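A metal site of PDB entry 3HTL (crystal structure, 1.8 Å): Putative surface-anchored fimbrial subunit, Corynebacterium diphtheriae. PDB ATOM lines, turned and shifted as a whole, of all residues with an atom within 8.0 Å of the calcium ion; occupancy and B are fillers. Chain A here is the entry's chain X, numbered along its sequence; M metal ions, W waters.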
ATOM      1  N   VAL A 152     -18.427  35.524   7.521  1.00  0.00           N
ATOM      2  CA  VAL A 152     -17.270  35.128   8.229  1.00  0.00           C
ATOM      3  C   VAL A 152     -17.107  33.615   8.065  1.00  0.00           C
ATOM      4  O   VAL A 152     -18.080  32.889   8.092  1.00  0.00           O
ATOM      5  CB  VAL A 152     -17.492  35.431   9.749  1.00  0.00           C
ATOM      6  CG1 VAL A 152     -16.368  34.901  10.574  1.00  0.00           C
ATOM      7  CG2 VAL A 152     -17.703  36.930   9.973  1.00  0.00           C
ATOM      8  N   ASP A 153     -15.884  33.140   7.887  1.00  0.00           N
ATOM      9  CA  ASP A 153     -15.617  31.692   7.899  1.00  0.00           C
ATOM     10  C   ASP A 153     -15.520  31.230   9.354  1.00  0.00           C
ATOM     11  O   ASP A 153     -14.564  31.629  10.036  1.00  0.00           O
ATOM     12  CB  ASP A 153     -14.302  31.381   7.192  1.00  0.00           C
ATOM     13  CG  ASP A 153     -14.002  29.894   7.108  1.00  0.00           C
ATOM     14  OD1 ASP A 153     -14.880  29.098   7.487  1.00  0.00           O
ATOM     15  OD2 ASP A 153     -12.892  29.525   6.683  1.00  0.00           O
ATOM     16  N   PRO A 154     -16.487  30.443   9.858  1.00  0.00           N
ATOM     17  CA  PRO A 154     -16.476  30.042  11.282  1.00  0.00           C
ATOM     18  C   PRO A 154     -15.518  28.921  11.623  1.00  0.00           C
ATOM     19  O   PRO A 154     -15.365  28.596  12.800  1.00  0.00           O
ATOM     20  CB  PRO A 154     -17.901  29.560  11.510  1.00  0.00           C
ATOM     21  CG  PRO A 154     -18.311  29.015  10.183  1.00  0.00           C
ATOM     22  CD  PRO A 154     -17.698  29.932   9.181  1.00  0.00           C
ATOM     23  N   ASP A 155     -14.907  28.294  10.620  1.00  0.00           N
ATOM     24  CA  ASP A 155     -13.994  27.184  10.862  1.00  0.00           C
ATOM     25  C   ASP A 155     -12.848  27.268   9.883  1.00  0.00           C
ATOM     26  O   ASP A 155     -13.032  27.010   8.702  1.00  0.00           O
ATOM     27  CB  ASP A 155     -14.749  25.863  10.716  1.00  0.00           C
ATOM     28  CG  ASP A 155     -13.902  24.676  11.143  1.00  0.00           C
ATOM     29  OD1 ASP A 155     -12.876  24.440  10.494  1.00  0.00           O
ATOM     30  OD2 ASP A 155     -14.275  23.975  12.102  1.00  0.00           O
ATOM     31  N   ALA A 156     -11.658  27.604  10.349  1.00  0.00           N
ATOM     32  CA  ALA A 156     -10.565  27.866   9.432  1.00  0.00           C
ATOM     33  C   ALA A 156      -9.772  26.617   9.018  1.00  0.00           C
ATOM     34  O   ALA A 156      -8.757  26.769   8.342  1.00  0.00           O
ATOM     35  CB  ALA A 156      -9.637  28.917  10.016  1.00  0.00           C
ATOM     36  N   THR A 157     -10.206  25.412   9.399  1.00  0.00           N
ATOM     37  CA  THR A 157      -9.576  24.159   8.969  1.00  0.00           C
ATOM     38  C   THR A 157      -9.444  24.080   7.437  1.00  0.00           C
ATOM     39  O   THR A 157      -8.415  23.629   6.924  1.00  0.00           O
ATOM     40  CB  THR A 157     -10.325  22.919   9.496  1.00  0.00           C
ATOM     41  OG1 THR A 157     -10.552  23.063  10.908  1.00  0.00           O
ATOM     42  CG2 THR A 157      -9.527  21.609   9.247  1.00  0.00           C
ATOM     43  N   GLN A 158     -10.466  24.510   6.729  1.00  0.00           N
ATOM     44  CA  GLN A 158     -10.359  24.736   5.261  1.00  0.00           C
ATOM     45  C   GLN A 158     -10.833  26.147   4.959  1.00  0.00           C
ATOM     46  O   GLN A 158     -11.870  26.592   5.461  1.00  0.00           O
ATOM     47  CB  GLN A 158     -11.188  23.715   4.466  1.00  0.00           C
ATOM     48  CG  GLN A 158     -11.139  23.877   2.953  1.00  0.00           C
ATOM     49  CD  GLN A 158     -11.873  22.719   2.290  1.00  0.00           C
ATOM     50  OE1 GLN A 158     -11.370  21.605   2.283  1.00  0.00           O
ATOM     51  NE2 GLN A 158     -13.080  22.975   1.820  1.00  0.00           N
ATOM     52  N   PRO A 159     -10.067  26.877   4.163  1.00  0.00           N
ATOM     53  CA  PRO A 159     -10.465  28.229   3.812  1.00  0.00           C
ATOM     54  C   PRO A 159     -11.867  28.347   3.251  1.00  0.00           C
ATOM     55  O   PRO A 159     -12.299  27.511   2.425  1.00  0.00           O
ATOM     56  CB  PRO A 159      -9.440  28.602   2.738  1.00  0.00           C
ATOM     57  CG  PRO A 159      -8.239  27.806   3.078  1.00  0.00           C
ATOM     58  CD  PRO A 159      -8.741  26.527   3.613  1.00  0.00           C
ATOM     59  N   GLY A 160     -12.612  29.357   3.697  1.00  0.00           N
ATOM     60  CA  GLY A 160     -13.886  29.631   3.130  1.00  0.00           C
ATOM     61  C   GLY A 160     -14.974  28.700   3.600  1.00  0.00           C
ATOM     62  O   GLY A 160     -14.828  27.993   4.634  1.00  0.00           O
ATOM     63  N   PHE A 161     -16.098  28.746   2.893  1.00  0.00           N
ATOM     64  CA  PHE A 161     -17.268  27.937   3.228  1.00  0.00           C
ATOM     65  C   PHE A 161     -17.826  27.284   1.923  1.00  0.00           C
ATOM     66  O   PHE A 161     -18.912  27.556   1.491  1.00  0.00           O
ATOM     67  CB  PHE A 161     -18.322  28.716   4.050  1.00  0.00           C
ATOM     68  CG  PHE A 161     -18.436  30.193   3.704  1.00  0.00           C
ATOM     69  CD1 PHE A 161     -17.736  31.150   4.446  1.00  0.00           C
ATOM     70  CD2 PHE A 161     -19.262  30.621   2.678  1.00  0.00           C
ATOM     71  CE1 PHE A 161     -17.857  32.502   4.137  1.00  0.00           C
ATOM     72  CE2 PHE A 161     -19.363  31.953   2.357  1.00  0.00           C
ATOM     73  CZ  PHE A 161     -18.670  32.903   3.098  1.00  0.00           C
ATOM     74  N   SER A 162     -17.020  26.392   1.367  1.00  0.00           N
ATOM     75  CA  SER A 162     -17.391  25.549   0.217  1.00  0.00           C
ATOM     76  C   SER A 162     -18.531  24.646   0.621  1.00  0.00           C
ATOM     77  O   SER A 162     -18.823  24.474   1.808  1.00  0.00           O
ATOM     78  CB  SER A 162     -16.200  24.714  -0.243  1.00  0.00           C
ATOM     79  OG  SER A 162     -15.260  25.485  -0.918  1.00  0.00           O
ATOM     80  N   GLU A 165     -19.520  22.768   4.214  1.00  0.00           N
ATOM     81  CA  GLU A 165     -19.086  23.545   5.376  1.00  0.00           C
ATOM     82  C   GLU A 165     -20.142  24.589   5.804  1.00  0.00           C
ATOM     83  O   GLU A 165     -21.095  24.821   5.082  1.00  0.00           O
ATOM     84  CB  GLU A 165     -17.782  24.288   5.049  1.00  0.00           C
ATOM     85  CG  GLU A 165     -16.573  23.395   4.724  1.00  0.00           C
ATOM     86  CD  GLU A 165     -15.270  23.854   5.413  1.00  0.00           C
ATOM     87  OE1 GLU A 165     -14.844  24.999   5.196  1.00  0.00           O
ATOM     88  OE2 GLU A 165     -14.672  23.052   6.182  1.00  0.00           O
ATOM     89  N   ASN A 166     -19.928  25.206   6.954  1.00  0.00           N
ATOM     90  CA  ASN A 166     -20.820  26.264   7.430  1.00  0.00           C
ATOM     91  C   ASN A 166     -20.326  27.678   7.091  1.00  0.00           C
ATOM     92  O   ASN A 166     -19.114  27.970   7.109  1.00  0.00           O
ATOM     93  CB  ASN A 166     -21.053  26.161   8.945  1.00  0.00           C
ATOM     94  CG  ASN A 166     -21.749  24.878   9.345  1.00  0.00           C
ATOM     95  OD1 ASN A 166     -22.732  24.444   8.731  1.00  0.00           O
ATOM     96  ND2 ASN A 166     -21.201  24.206  10.352  1.00  0.00           N
ATOM     97  N   VAL A 167     -21.298  28.522   6.810  1.00  0.00           N
ATOM     98  CA  VAL A 167     -21.067  29.971   6.684  1.00  0.00           C
ATOM     99  C   VAL A 167     -21.592  30.645   7.961  1.00  0.00           C
ATOM    100  O   VAL A 167     -22.538  30.156   8.598  1.00  0.00           O
ATOM    101  CB  VAL A 167     -21.716  30.583   5.401  1.00  0.00           C
ATOM    102  CG1 VAL A 167     -23.244  30.482   5.413  1.00  0.00           C
ATOM    103  CG2 VAL A 167     -21.309  32.013   5.237  1.00  0.00           C
ATOM    104  N   HIS A 368     -16.081  27.526  -2.821  1.00  0.00           N
ATOM    105  CA  HIS A 368     -16.245  28.936  -2.437  1.00  0.00           C
ATOM    106  C   HIS A 368     -14.931  29.688  -2.652  1.00  0.00           C
ATOM    107  O   HIS A 368     -13.890  29.391  -2.051  1.00  0.00           O
ATOM    108  CB  HIS A 368     -16.733  29.072  -0.999  1.00  0.00           C
ATOM    109  CG  HIS A 368     -16.659  30.456  -0.464  1.00  0.00           C
ATOM    110  ND1 HIS A 368     -16.141  30.740   0.781  1.00  0.00           N
ATOM    111  CD2 HIS A 368     -16.987  31.653  -1.026  1.00  0.00           C
ATOM    112  CE1 HIS A 368     -16.190  32.047   0.989  1.00  0.00           C
ATOM    113  NE2 HIS A 368     -16.692  32.621  -0.090  1.00  0.00           N
HETATM  114 CA    CA M   1     -13.874  27.062   6.517  1.00  0.00          CA
HETATM  115  O   HOH W   1     -16.564  26.561   7.534  1.00  0.00           O
HETATM  116  O   HOH W   2     -13.353  24.370   7.711  1.00  0.00           O
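The side-chain hydroxyl of Thr 157 is in hydrogen-bond range of the side-chain carboxylate of Asp 155 (2.7 Å).
Water W2 lies within hydrogen-bond range of OE2 of Glu 165 (2.4 Å), OD1 of Asp 155 (2.8 Å) and N of Gln 158 (3.1 Å).
Five residues have an atom within 4 Å of the calcium ion: Asp 153, Asp 155, Gln 158, Gly 160 and Glu 165. The nearest printed residue that does not touch the calcium ion is Pro 159 (4.04 Å).
The calcium ion is bound by O of Gly 160 (2.3 Å), O of Gln 158 (2.3 Å), O of Asp 155 (2.3 Å), OD1 of Asp 153 (2.5 Å), OE1 of Glu 165 (2.6 Å) and OD2 of Asp 153 (2.7 Å). Slightly farther from the calcium ion lies water W1 (2.9 Å). Slightly farther from the calcium ion lies water W2 (3.0 Å).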
